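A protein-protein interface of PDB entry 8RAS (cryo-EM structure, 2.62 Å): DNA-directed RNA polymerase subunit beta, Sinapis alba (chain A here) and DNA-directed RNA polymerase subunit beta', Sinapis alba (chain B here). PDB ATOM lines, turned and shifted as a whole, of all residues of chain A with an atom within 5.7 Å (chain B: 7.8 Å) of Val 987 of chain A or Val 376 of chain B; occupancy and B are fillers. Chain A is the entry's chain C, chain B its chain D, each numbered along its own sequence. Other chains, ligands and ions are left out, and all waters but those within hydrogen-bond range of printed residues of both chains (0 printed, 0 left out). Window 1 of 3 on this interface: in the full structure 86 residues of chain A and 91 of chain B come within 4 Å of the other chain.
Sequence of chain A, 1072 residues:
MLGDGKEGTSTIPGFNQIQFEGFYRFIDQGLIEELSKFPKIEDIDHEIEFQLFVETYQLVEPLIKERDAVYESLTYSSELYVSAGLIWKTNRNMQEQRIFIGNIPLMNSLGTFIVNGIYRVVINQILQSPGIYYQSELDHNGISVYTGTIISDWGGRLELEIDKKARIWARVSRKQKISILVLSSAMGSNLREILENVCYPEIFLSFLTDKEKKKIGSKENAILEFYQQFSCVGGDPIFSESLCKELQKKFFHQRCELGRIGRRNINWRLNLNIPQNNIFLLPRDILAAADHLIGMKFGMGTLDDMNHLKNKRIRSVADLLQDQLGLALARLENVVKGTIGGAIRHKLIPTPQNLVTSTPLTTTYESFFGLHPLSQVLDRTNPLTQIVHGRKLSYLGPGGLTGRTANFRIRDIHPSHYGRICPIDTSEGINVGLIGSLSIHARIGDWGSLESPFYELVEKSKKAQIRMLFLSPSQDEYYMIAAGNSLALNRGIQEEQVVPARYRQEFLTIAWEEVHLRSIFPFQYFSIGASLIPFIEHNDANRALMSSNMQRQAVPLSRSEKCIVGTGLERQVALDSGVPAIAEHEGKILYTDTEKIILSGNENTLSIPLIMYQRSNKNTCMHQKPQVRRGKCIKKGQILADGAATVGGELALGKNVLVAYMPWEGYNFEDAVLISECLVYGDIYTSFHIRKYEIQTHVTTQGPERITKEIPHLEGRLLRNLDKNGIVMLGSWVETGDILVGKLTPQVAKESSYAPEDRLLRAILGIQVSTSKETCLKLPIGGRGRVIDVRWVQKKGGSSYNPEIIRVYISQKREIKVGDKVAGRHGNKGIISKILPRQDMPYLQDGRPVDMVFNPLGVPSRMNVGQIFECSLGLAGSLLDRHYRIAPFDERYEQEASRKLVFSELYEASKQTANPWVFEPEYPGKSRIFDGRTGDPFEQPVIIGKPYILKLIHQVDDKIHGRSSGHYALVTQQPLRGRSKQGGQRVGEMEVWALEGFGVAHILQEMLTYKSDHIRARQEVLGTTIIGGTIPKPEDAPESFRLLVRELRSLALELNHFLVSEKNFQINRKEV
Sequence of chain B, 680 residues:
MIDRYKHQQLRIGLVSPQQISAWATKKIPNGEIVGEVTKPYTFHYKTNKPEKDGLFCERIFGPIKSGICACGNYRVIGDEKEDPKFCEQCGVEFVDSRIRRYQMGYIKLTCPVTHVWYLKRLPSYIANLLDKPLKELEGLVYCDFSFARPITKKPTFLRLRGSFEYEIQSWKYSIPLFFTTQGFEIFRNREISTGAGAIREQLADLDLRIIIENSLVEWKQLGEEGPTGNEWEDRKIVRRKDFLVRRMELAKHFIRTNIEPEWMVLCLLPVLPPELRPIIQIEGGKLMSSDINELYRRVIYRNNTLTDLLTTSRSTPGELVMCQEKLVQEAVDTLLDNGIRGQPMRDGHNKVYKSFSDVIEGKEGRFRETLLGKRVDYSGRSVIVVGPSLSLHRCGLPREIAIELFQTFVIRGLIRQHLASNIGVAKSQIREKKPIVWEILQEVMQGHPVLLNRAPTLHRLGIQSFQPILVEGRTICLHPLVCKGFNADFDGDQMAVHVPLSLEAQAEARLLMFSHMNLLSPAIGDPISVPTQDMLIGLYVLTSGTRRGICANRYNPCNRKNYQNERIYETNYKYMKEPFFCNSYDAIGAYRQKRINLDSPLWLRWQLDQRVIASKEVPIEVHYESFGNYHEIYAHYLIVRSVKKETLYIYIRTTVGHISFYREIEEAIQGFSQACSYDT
OD1 of Asp 377 of chain B is in salt-bridge range of NH2 of Arg 963 of chain A. The backbone NH (N) of Tyr 378 of chain B lies close to the backbone carbonyl oxygen (O) of Arg 963 of chain A (3.3 Å). N of Arg 963 of chain A is in hydrogen-bond range of O of Ser 379 of chain B. O of Gly 984 of chain A lies within hydrogen-bond range of NE of Arg 375 of chain B (3.2 Å). The backbone NH of Val 376 of chain B sits at hydrogen-bond distance from the backbone carbonyl oxygen of Gln 985 of chain A. The backbone NH (N) of Gln 985 of chain A sits at hydrogen-bond distance from the side-chain hydroxyl (OG) of Ser 379 of chain B (2.9 Å). NH2 of Arg 986 of chain A lies within salt-bridge range of OE2 of Glu 369 of chain B (3.6 Å). The guanidinium group (NH1) of Arg 986 of chain A sits at hydrogen-bond distance from the backbone carbonyl oxygen (O) of Gly 373 of chain B. The backbone carbonyl oxygen (O) of Lys 374 of chain B lies within hydrogen-bond range of the backbone NH (N) of Val 987 of chain A (2.7 Å). The side-chain carboxylate (OE2) of Glu 991 of chain A sits at hydrogen-bond distance from the side-chain amide nitrogen (ND2) of Asn 453 of chain B, at 3.3 Å. The side-chain amino group (NZ) of Lys 374 of chain B sits at hydrogen-bond distance from the backbone carbonyl oxygen (O) of Leu 1008 of chain A, 3.4 Å away. The backbone carbonyl oxygen of Lys 1011 of chain A sits at hydrogen-bond distance from the backbone NH of Asp 377 of chain B (2.8 Å). NZ of Lys 1011 of chain A is in hydrogen-bond range of O of Val 499 of chain B (2.8 Å). The side-chain hydroxyl of Ser 1012 of chain A is in hydrogen-bond range of the backbone carbonyl oxygen of Arg 375 of chain B (2.5 Å).
The backbone carbonyl oxygen (O) of Asn 453 of chain B is in hydrogen-bond range of the backbone NH (N) of Ala 496 of chain B (2.9 Å).
Printed residues of chain B within 4 Å of Arg 986 of chain A: Glu 369 (3.1 Å), Gly 373 (2.9 Å), Lys 374 (3.6 Å) and Arg 375 (3.7 Å). Val 987 of chain A touches four residues of chain B. Of chain A, only Pro 975 (3.9 Å), Gly 984 (3.4 Å), Gln 985 (3.1 Å), Val 987 (3.9 Å), Met 1007 (3.3 Å) and Lys 1011 (3.4 Å) come within 4 Å of Val 376 of chain B. Of the printed residues of chain A, Tyr 378 of chain B touches Arg 963 (3.1 Å). The nearest residue of chain A that does not touch Val 376 of chain B is Ser 1012 of chain A (4.6 Å). The nearest printed residue of chain A that does not touch Gly 380 of chain B is Arg 963 of chain A (4.7 Å).
Of the 17 printed residues of chain A, 14 touch a printed residue of chain B. Hydrophobic or aromatic side chains of chain B that line the printed part of chain A: Leu 372, Val 376, Ile 463 and His 498. Among the printed residues, Asp or Glu carboxylates within 4 Å of a Lys or Arg side-chain nitrogen of the other chain: Arg 963 of chain A with Asp 377 of chain B (2.7 Å) and Arg 986 of chain A with Glu 369 of chain B (3.6 Å).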
ATOM      1  N   ARG A 963       2.637  16.517 -17.966  1.00  0.00           N
ATOM      2  CA  ARG A 963       3.899  15.910 -18.364  1.00  0.00           C
ATOM      3  C   ARG A 963       4.016  15.929 -19.878  1.00  0.00           C
ATOM      4  O   ARG A 963       3.054  15.611 -20.579  1.00  0.00           O
ATOM      5  CB  ARG A 963       4.004  14.473 -17.842  1.00  0.00           C
ATOM      6  CG  ARG A 963       4.796  13.539 -18.736  1.00  0.00           C
ATOM      7  CD  ARG A 963       5.448  12.431 -17.938  1.00  0.00           C
ATOM      8  NE  ARG A 963       6.429  11.695 -18.723  1.00  0.00           N
ATOM      9  CZ  ARG A 963       7.461  11.043 -18.208  1.00  0.00           C
ATOM     10  NH1 ARG A 963       7.678  11.015 -16.903  1.00  0.00           N
ATOM     11  NH2 ARG A 963       8.297  10.404 -19.019  1.00  0.00           N
ATOM     12  N   PRO A 975       7.433   5.605 -18.730  1.00  0.00           N
ATOM     13  CA  PRO A 975       7.428   6.806 -17.888  1.00  0.00           C
ATOM     14  C   PRO A 975       7.114   6.468 -16.440  1.00  0.00           C
ATOM     15  O   PRO A 975       6.381   5.522 -16.143  1.00  0.00           O
ATOM     16  CB  PRO A 975       6.327   7.669 -18.511  1.00  0.00           C
ATOM     17  CG  PRO A 975       6.270   7.234 -19.922  1.00  0.00           C
ATOM     18  CD  PRO A 975       6.594   5.772 -19.928  1.00  0.00           C
ATOM     19  N   GLY A 983       5.665  11.893 -13.281  1.00  0.00           N
ATOM     20  CA  GLY A 983       5.337  10.728 -14.070  1.00  0.00           C
ATOM     21  C   GLY A 983       4.144  10.950 -14.976  1.00  0.00           C
ATOM     22  O   GLY A 983       3.479  11.984 -14.951  1.00  0.00           O
ATOM     23  N   GLY A 984       3.872   9.936 -15.799  1.00  0.00           N
ATOM     24  CA  GLY A 984       2.788   9.985 -16.752  1.00  0.00           C
ATOM     25  C   GLY A 984       1.551   9.238 -16.277  1.00  0.00           C
ATOM     26  O   GLY A 984       1.530   8.588 -15.235  1.00  0.00           O
ATOM     27  N   GLN A 985       0.499   9.346 -17.082  1.00  0.00           N
ATOM     28  CA  GLN A 985      -0.771   8.697 -16.791  1.00  0.00           C
ATOM     29  C   GLN A 985      -0.806   7.313 -17.423  1.00  0.00           C
ATOM     30  O   GLN A 985      -0.366   7.124 -18.560  1.00  0.00           O
ATOM     31  CB  GLN A 985      -1.940   9.535 -17.309  1.00  0.00           C
ATOM     32  CG  GLN A 985      -1.945  10.969 -16.814  1.00  0.00           C
ATOM     33  CD  GLN A 985      -2.039  11.066 -15.308  1.00  0.00           C
ATOM     34  OE1 GLN A 985      -2.848  10.386 -14.681  1.00  0.00           O
ATOM     35  NE2 GLN A 985      -1.208  11.915 -14.717  1.00  0.00           N
ATOM     36  N   ARG A 986      -1.334   6.348 -16.679  1.00  0.00           N
ATOM     37  CA  ARG A 986      -1.391   4.975 -17.158  1.00  0.00           C
ATOM     38  C   ARG A 986      -2.598   4.771 -18.061  1.00  0.00           C
ATOM     39  O   ARG A 986      -3.707   5.217 -17.746  1.00  0.00           O
ATOM     40  CB  ARG A 986      -1.446   3.995 -15.988  1.00  0.00           C
ATOM     41  CG  ARG A 986      -1.391   2.544 -16.418  1.00  0.00           C
ATOM     42  CD  ARG A 986      -1.317   1.611 -15.232  1.00  0.00           C
ATOM     43  NE  ARG A 986      -1.804   0.279 -15.569  1.00  0.00           N
ATOM     44  CZ  ARG A 986      -1.098  -0.636 -16.217  1.00  0.00           C
ATOM     45  NH1 ARG A 986       0.141  -0.400 -16.616  1.00  0.00           N
ATOM     46  NH2 ARG A 986      -1.649  -1.819 -16.472  1.00  0.00           N
ATOM     47  N   VAL A 987      -2.378   4.099 -19.185  1.00  0.00           N
ATOM     48  CA  VAL A 987      -3.455   3.666 -20.067  1.00  0.00           C
ATOM     49  C   VAL A 987      -3.621   2.173 -19.807  1.00  0.00           C
ATOM     50  O   VAL A 987      -2.928   1.334 -20.382  1.00  0.00           O
ATOM     51  CB  VAL A 987      -3.154   3.974 -21.532  1.00  0.00           C
ATOM     52  CG1 VAL A 987      -4.290   3.496 -22.415  1.00  0.00           C
ATOM     53  CG2 VAL A 987      -2.923   5.462 -21.715  1.00  0.00           C
ATOM     54  N   GLY A 988      -4.555   1.836 -18.920  1.00  0.00           N
ATOM     55  CA  GLY A 988      -4.754   0.464 -18.515  1.00  0.00           C
ATOM     56  C   GLY A 988      -5.453  -0.359 -19.574  1.00  0.00           C
ATOM     57  O   GLY A 988      -5.812   0.119 -20.650  1.00  0.00           O
ATOM     58  N   GLU A 989      -5.651  -1.638 -19.250  1.00  0.00           N
ATOM     59  CA  GLU A 989      -6.278  -2.548 -20.203  1.00  0.00           C
ATOM     60  C   GLU A 989      -7.733  -2.179 -20.464  1.00  0.00           C
ATOM     61  O   GLU A 989      -8.245  -2.435 -21.559  1.00  0.00           O
ATOM     62  CB  GLU A 989      -6.161  -3.989 -19.704  1.00  0.00           C
ATOM     63  CG  GLU A 989      -7.420  -4.546 -19.071  1.00  0.00           C
ATOM     64  CD  GLU A 989      -7.158  -5.790 -18.250  1.00  0.00           C
ATOM     65  OE1 GLU A 989      -6.541  -6.736 -18.781  1.00  0.00           O
ATOM     66  OE2 GLU A 989      -7.570  -5.821 -17.071  1.00  0.00           O
ATOM     67  N   GLU A 991      -8.781   0.939 -20.600  1.00  0.00           N
ATOM     68  CA  GLU A 991      -8.667   2.033 -21.557  1.00  0.00           C
ATOM     69  C   GLU A 991      -8.335   1.521 -22.951  1.00  0.00           C
ATOM     70  O   GLU A 991      -8.756   2.119 -23.946  1.00  0.00           O
ATOM     71  CB  GLU A 991      -7.606   3.027 -21.091  1.00  0.00           C
ATOM     72  CG  GLU A 991      -8.079   4.007 -20.034  1.00  0.00           C
ATOM     73  CD  GLU A 991      -8.158   3.385 -18.653  1.00  0.00           C
ATOM     74  OE1 GLU A 991      -7.536   2.325 -18.439  1.00  0.00           O
ATOM     75  OE2 GLU A 991      -8.840   3.960 -17.779  1.00  0.00           O
ATOM     76  N   VAL A 992      -7.575   0.429 -23.041  1.00  0.00           N
ATOM     77  CA  VAL A 992      -7.255  -0.157 -24.339  1.00  0.00           C
ATOM     78  C   VAL A 992      -8.503  -0.755 -24.976  1.00  0.00           C
ATOM     79  O   VAL A 992      -8.683  -0.690 -26.199  1.00  0.00           O
ATOM     80  CB  VAL A 992      -6.130  -1.197 -24.190  1.00  0.00           C
ATOM     81  CG1 VAL A 992      -5.870  -1.902 -25.508  1.00  0.00           C
ATOM     82  CG2 VAL A 992      -4.860  -0.530 -23.687  1.00  0.00           C
ATOM     83  N   LEU A 995     -10.467   2.065 -26.671  1.00  0.00           N
ATOM     84  CA  LEU A 995      -9.868   2.463 -27.940  1.00  0.00           C
ATOM     85  C   LEU A 995     -10.118   1.421 -29.020  1.00  0.00           C
ATOM     86  O   LEU A 995     -10.344   1.768 -30.184  1.00  0.00           O
ATOM     87  CB  LEU A 995      -8.373   2.704 -27.757  1.00  0.00           C
ATOM     88  CG  LEU A 995      -8.008   3.761 -26.716  1.00  0.00           C
ATOM     89  CD1 LEU A 995      -6.510   3.818 -26.537  1.00  0.00           C
ATOM     90  CD2 LEU A 995      -8.553   5.115 -27.122  1.00  0.00           C
ATOM     91  N   LEU A1004      -4.040   4.049 -30.430  1.00  0.00           N
ATOM     92  CA  LEU A1004      -3.568   2.992 -29.543  1.00  0.00           C
ATOM     93  C   LEU A1004      -2.080   2.726 -29.734  1.00  0.00           C
ATOM     94  O   LEU A1004      -1.347   2.536 -28.757  1.00  0.00           O
ATOM     95  CB  LEU A1004      -4.377   1.718 -29.781  1.00  0.00           C
ATOM     96  CG  LEU A1004      -4.166   0.553 -28.814  1.00  0.00           C
ATOM     97  CD1 LEU A1004      -4.100   1.048 -27.380  1.00  0.00           C
ATOM     98  CD2 LEU A1004      -5.272  -0.474 -28.978  1.00  0.00           C
ATOM     99  N   MET A1007       0.234   5.352 -27.989  1.00  0.00           N
ATOM    100  CA  MET A1007       0.373   5.192 -26.552  1.00  0.00           C
ATOM    101  C   MET A1007       0.924   3.830 -26.163  1.00  0.00           C
ATOM    102  O   MET A1007       1.068   3.551 -24.969  1.00  0.00           O
ATOM    103  CB  MET A1007      -0.978   5.436 -25.876  1.00  0.00           C
ATOM    104  CG  MET A1007      -1.342   6.913 -25.792  1.00  0.00           C
ATOM    105  SD  MET A1007      -3.070   7.235 -25.404  1.00  0.00           S
ATOM    106  CE  MET A1007      -3.698   5.569 -25.277  1.00  0.00           C
ATOM    107  N   LEU A1008       1.232   2.977 -27.137  1.00  0.00           N
ATOM    108  CA  LEU A1008       1.850   1.689 -26.863  1.00  0.00           C
ATOM    109  C   LEU A1008       3.332   1.649 -27.192  1.00  0.00           C
ATOM    110  O   LEU A1008       4.067   0.887 -26.555  1.00  0.00           O
ATOM    111  CB  LEU A1008       1.142   0.575 -27.642  1.00  0.00           C
ATOM    112  CG  LEU A1008      -0.190   0.062 -27.094  1.00  0.00           C
ATOM    113  CD1 LEU A1008      -0.701  -1.088 -27.941  1.00  0.00           C
ATOM    114  CD2 LEU A1008      -0.060  -0.357 -25.639  1.00  0.00           C
ATOM    115  N   LYS A1011       5.118   6.739 -27.073  1.00  0.00           N
ATOM    116  CA  LYS A1011       4.844   7.558 -25.908  1.00  0.00           C
ATOM    117  C   LYS A1011       5.168   6.842 -24.609  1.00  0.00           C
ATOM    118  O   LYS A1011       5.162   7.482 -23.553  1.00  0.00           O
ATOM    119  CB  LYS A1011       3.377   8.012 -25.899  1.00  0.00           C
ATOM    120  CG  LYS A1011       3.116   9.239 -26.755  1.00  0.00           C
ATOM    121  CD  LYS A1011       1.685   9.285 -27.255  1.00  0.00           C
ATOM    122  CE  LYS A1011       0.780  10.002 -26.274  1.00  0.00           C
ATOM    123  NZ  LYS A1011      -0.511  10.390 -26.903  1.00  0.00           N
ATOM    124  N   SER A1012       5.450   5.539 -24.653  1.00  0.00           N
ATOM    125  CA  SER A1012       5.734   4.785 -23.439  1.00  0.00           C
ATOM    126  C   SER A1012       7.151   4.229 -23.393  1.00  0.00           C
ATOM    127  O   SER A1012       7.915   4.595 -22.495  1.00  0.00           O
ATOM    128  CB  SER A1012       4.711   3.651 -23.300  1.00  0.00           C
ATOM    129  OG  SER A1012       4.707   3.136 -21.982  1.00  0.00           O
ATOM    130  N   GLU B 369       0.502  -6.506 -16.642  1.00  0.00           N
ATOM    131  CA  GLU B 369       0.800  -5.186 -16.100  1.00  0.00           C
ATOM    132  C   GLU B 369       1.685  -4.344 -17.003  1.00  0.00           C
ATOM    133  O   GLU B 369       1.440  -3.146 -17.150  1.00  0.00           O
ATOM    134  CB  GLU B 369       1.465  -5.315 -14.723  1.00  0.00           C
ATOM    135  CG  GLU B 369       1.291  -4.097 -13.834  1.00  0.00           C
ATOM    136  CD  GLU B 369      -0.073  -4.046 -13.176  1.00  0.00           C
ATOM    137  OE1 GLU B 369      -0.496  -5.073 -12.605  1.00  0.00           O
ATOM    138  OE2 GLU B 369      -0.722  -2.980 -13.229  1.00  0.00           O
ATOM    139  N   LEU B 371       2.573  -5.199 -20.400  1.00  0.00           N
ATOM    140  CA  LEU B 371       2.249  -5.322 -21.816  1.00  0.00           C
ATOM    141  C   LEU B 371       0.820  -4.915 -22.146  1.00  0.00           C
ATOM    142  O   LEU B 371       0.589  -4.284 -23.181  1.00  0.00           O
ATOM    143  CB  LEU B 371       2.489  -6.760 -22.284  1.00  0.00           C
ATOM    144  CG  LEU B 371       3.852  -7.350 -21.915  1.00  0.00           C
ATOM    145  CD1 LEU B 371       3.979  -8.773 -22.421  1.00  0.00           C
ATOM    146  CD2 LEU B 371       4.967  -6.486 -22.465  1.00  0.00           C
ATOM    147  N   LEU B 372      -0.146  -5.262 -21.298  1.00  0.00           N
ATOM    148  CA  LEU B 372      -1.539  -4.927 -21.567  1.00  0.00           C
ATOM    149  C   LEU B 372      -1.887  -3.491 -21.199  1.00  0.00           C
ATOM    150  O   LEU B 372      -2.946  -3.004 -21.610  1.00  0.00           O
ATOM    151  CB  LEU B 372      -2.466  -5.890 -20.821  1.00  0.00           C
ATOM    152  CG  LEU B 372      -2.506  -7.332 -21.330  1.00  0.00           C
ATOM    153  CD1 LEU B 372      -3.716  -8.063 -20.774  1.00  0.00           C
ATOM    154  CD2 LEU B 372      -2.500  -7.376 -22.849  1.00  0.00           C
ATOM    155  N   GLY B 373      -1.033  -2.808 -20.445  1.00  0.00           N
ATOM    156  CA  GLY B 373      -1.255  -1.418 -20.099  1.00  0.00           C
ATOM    157  C   GLY B 373       0.050  -0.679 -19.897  1.00  0.00           C
ATOM    158  O   GLY B 373       0.989  -1.224 -19.313  1.00  0.00           O
ATOM    159  N   LYS B 374       0.127   0.561 -20.372  1.00  0.00           N
ATOM    160  CA  LYS B 374       1.366   1.322 -20.347  1.00  0.00           C
ATOM    161  C   LYS B 374       1.120   2.727 -19.820  1.00  0.00           C
ATOM    162  O   LYS B 374       0.048   3.305 -20.017  1.00  0.00           O
ATOM    163  CB  LYS B 374       1.996   1.409 -21.745  1.00  0.00           C
ATOM    164  CG  LYS B 374       2.099   0.085 -22.479  1.00  0.00           C
ATOM    165  CD  LYS B 374       3.385  -0.004 -23.277  1.00  0.00           C
ATOM    166  CE  LYS B 374       3.563  -1.382 -23.881  1.00  0.00           C
ATOM    167  NZ  LYS B 374       4.953  -1.597 -24.366  1.00  0.00           N
ATOM    168  N   ARG B 375       2.128   3.269 -19.142  1.00  0.00           N
ATOM    169  CA  ARG B 375       2.151   4.687 -18.815  1.00  0.00           C
ATOM    170  C   ARG B 375       2.720   5.460 -19.995  1.00  0.00           C
ATOM    171  O   ARG B 375       3.651   5.000 -20.659  1.00  0.00           O
ATOM    172  CB  ARG B 375       2.988   4.939 -17.563  1.00  0.00           C
ATOM    173  CG  ARG B 375       2.755   3.931 -16.455  1.00  0.00           C
ATOM    174  CD  ARG B 375       3.142   4.499 -15.104  1.00  0.00           C
ATOM    175  NE  ARG B 375       2.166   5.468 -14.622  1.00  0.00           N
ATOM    176  CZ  ARG B 375       1.219   5.197 -13.735  1.00  0.00           C
ATOM    177  NH1 ARG B 375       1.088   3.990 -13.211  1.00  0.00           N
ATOM    178  NH2 ARG B 375       0.385   6.162 -13.362  1.00  0.00           N
ATOM    179  N   VAL B 376       2.156   6.637 -20.263  1.00  0.00           N
ATOM    180  CA  VAL B 376       2.438   7.349 -21.499  1.00  0.00           C
ATOM    181  C   VAL B 376       2.898   8.768 -21.197  1.00  0.00           C
ATOM    182  O   VAL B 376       2.631   9.328 -20.132  1.00  0.00           O
ATOM    183  CB  VAL B 376       1.215   7.379 -22.439  1.00  0.00           C
ATOM    184  CG1 VAL B 376       0.787   5.967 -22.787  1.00  0.00           C
ATOM    185  CG2 VAL B 376       0.071   8.140 -21.796  1.00  0.00           C
ATOM    186  N   ASP B 377       3.611   9.342 -22.164  1.00  0.00           N
ATOM    187  CA  ASP B 377       4.026  10.734 -22.118  1.00  0.00           C
ATOM    188  C   ASP B 377       2.910  11.627 -22.651  1.00  0.00           C
ATOM    189  O   ASP B 377       1.878  11.156 -23.136  1.00  0.00           O
ATOM    190  CB  ASP B 377       5.306  10.938 -22.925  1.00  0.00           C
ATOM    191  CG  ASP B 377       6.504  10.268 -22.296  1.00  0.00           C
ATOM    192  OD1 ASP B 377       6.597  10.260 -21.052  1.00  0.00           O
ATOM    193  OD2 ASP B 377       7.358   9.754 -23.046  1.00  0.00           O
ATOM    194  N   TYR B 378       3.129  12.941 -22.569  1.00  0.00           N
ATOM    195  CA  TYR B 378       2.177  13.934 -23.068  1.00  0.00           C
ATOM    196  C   TYR B 378       0.794  13.726 -22.460  1.00  0.00           C
ATOM    197  O   TYR B 378      -0.228  13.777 -23.147  1.00  0.00           O
ATOM    198  CB  TYR B 378       2.119  13.919 -24.596  1.00  0.00           C
ATOM    199  CG  TYR B 378       3.464  14.141 -25.246  1.00  0.00           C
ATOM    200  CD1 TYR B 378       3.936  15.422 -25.486  1.00  0.00           C
ATOM    201  CD2 TYR B 378       4.265  13.069 -25.610  1.00  0.00           C
ATOM    202  CE1 TYR B 378       5.165  15.630 -26.074  1.00  0.00           C
ATOM    203  CE2 TYR B 378       5.497  13.268 -26.198  1.00  0.00           C
ATOM    204  CZ  TYR B 378       5.941  14.550 -26.429  1.00  0.00           C
ATOM    205  OH  TYR B 378       7.167  14.753 -27.016  1.00  0.00           O
ATOM    206  N   SER B 379       0.763  13.486 -21.153  1.00  0.00           N
ATOM    207  CA  SER B 379      -0.473  13.233 -20.433  1.00  0.00           C
ATOM    208  C   SER B 379      -0.512  14.070 -19.162  1.00  0.00           C
ATOM    209  O   SER B 379       0.525  14.384 -18.574  1.00  0.00           O
ATOM    210  CB  SER B 379      -0.626  11.748 -20.088  1.00  0.00           C
ATOM    211  OG  SER B 379       0.441  11.303 -19.270  1.00  0.00           O
ATOM    212  N   GLY B 380      -1.723  14.427 -18.745  1.00  0.00           N
ATOM    213  CA  GLY B 380      -1.909  15.247 -17.565  1.00  0.00           C
ATOM    214  C   GLY B 380      -3.073  14.804 -16.706  1.00  0.00           C
ATOM    215  O   GLY B 380      -3.707  13.785 -16.992  1.00  0.00           O
ATOM    216  N   ASN B 453     -10.377  11.148 -20.124  1.00  0.00           N
ATOM    217  CA  ASN B 453     -10.621   9.781 -19.672  1.00  0.00           C
ATOM    218  C   ASN B 453     -10.813   9.777 -18.165  1.00  0.00           C
ATOM    219  O   ASN B 453      -9.940  10.249 -17.431  1.00  0.00           O
ATOM    220  CB  ASN B 453      -9.458   8.873 -20.071  1.00  0.00           C
ATOM    221  CG  ASN B 453      -9.512   7.523 -19.392  1.00  0.00           C
ATOM    222  OD1 ASN B 453     -10.545   6.856 -19.393  1.00  0.00           O
ATOM    223  ND2 ASN B 453      -8.395   7.112 -18.807  1.00  0.00           N
ATOM    224  N   ILE B 463     -13.780   7.297 -22.573  1.00  0.00           N
ATOM    225  CA  ILE B 463     -12.765   8.193 -23.111  1.00  0.00           C
ATOM    226  C   ILE B 463     -13.337   8.851 -24.358  1.00  0.00           C
ATOM    227  O   ILE B 463     -13.846   8.165 -25.250  1.00  0.00           O
ATOM    228  CB  ILE B 463     -11.448   7.457 -23.428  1.00  0.00           C
ATOM    229  CG1 ILE B 463     -10.535   8.334 -24.284  1.00  0.00           C
ATOM    230  CG2 ILE B 463     -11.718   6.137 -24.114  1.00  0.00           C
ATOM    231  CD1 ILE B 463      -9.115   7.835 -24.362  1.00  0.00           C
ATOM    232  N   ALA B 496      -7.837  12.230 -16.865  1.00  0.00           N
ATOM    233  CA  ALA B 496      -6.557  12.242 -17.553  1.00  0.00           C
ATOM    234  C   ALA B 496      -6.738  12.812 -18.952  1.00  0.00           C
ATOM    235  O   ALA B 496      -7.764  12.586 -19.598  1.00  0.00           O
ATOM    236  CB  ALA B 496      -5.964  10.835 -17.630  1.00  0.00           C
ATOM    237  N   VAL B 497      -5.738  13.557 -19.415  1.00  0.00           N
ATOM    238  CA  VAL B 497      -5.755  14.183 -20.730  1.00  0.00           C
ATOM    239  C   VAL B 497      -4.600  13.624 -21.545  1.00  0.00           C
ATOM    240  O   VAL B 497      -3.487  13.473 -21.033  1.00  0.00           O
ATOM    241  CB  VAL B 497      -5.658  15.719 -20.637  1.00  0.00           C
ATOM    242  CG1 VAL B 497      -6.057  16.355 -21.955  1.00  0.00           C
ATOM    243  CG2 VAL B 497      -6.526  16.238 -19.512  1.00  0.00           C
ATOM    244  N   HIS B 498      -4.868  13.311 -22.809  1.00  0.00           N
ATOM    245  CA  HIS B 498      -3.855  12.797 -23.718  1.00  0.00           C
ATOM    246  C   HIS B 498      -3.892  13.588 -25.016  1.00  0.00           C
ATOM    247  O   HIS B 498      -4.955  14.025 -25.463  1.00  0.00           O
ATOM    248  CB  HIS B 498      -4.062  11.305 -24.007  1.00  0.00           C
ATOM    249  CG  HIS B 498      -4.220  10.466 -22.777  1.00  0.00           C
ATOM    250  ND1 HIS B 498      -3.159   9.836 -22.166  1.00  0.00           N
ATOM    251  CD2 HIS B 498      -5.316  10.148 -22.049  1.00  0.00           C
ATOM    252  CE1 HIS B 498      -3.592   9.170 -21.112  1.00  0.00           C
ATOM    253  NE2 HIS B 498      -4.898   9.343 -21.019  1.00  0.00           N
ATOM    254  N   VAL B 499      -2.723  13.765 -25.616  1.00  0.00           N
ATOM    255  CA  VAL B 499      -2.559  14.544 -26.840  1.00  0.00           C
ATOM    256  C   VAL B 499      -2.163  13.591 -27.962  1.00  0.00           C
ATOM    257  O   VAL B 499      -1.085  12.986 -27.900  1.00  0.00           O
ATOM    258  CB  VAL B 499      -1.508  15.653 -26.669  1.00  0.00           C
ATOM    259  CG1 VAL B 499      -1.139  16.245 -28.016  1.00  0.00           C
ATOM    260  CG2 VAL B 499      -2.027  16.731 -25.746  1.00  0.00           C
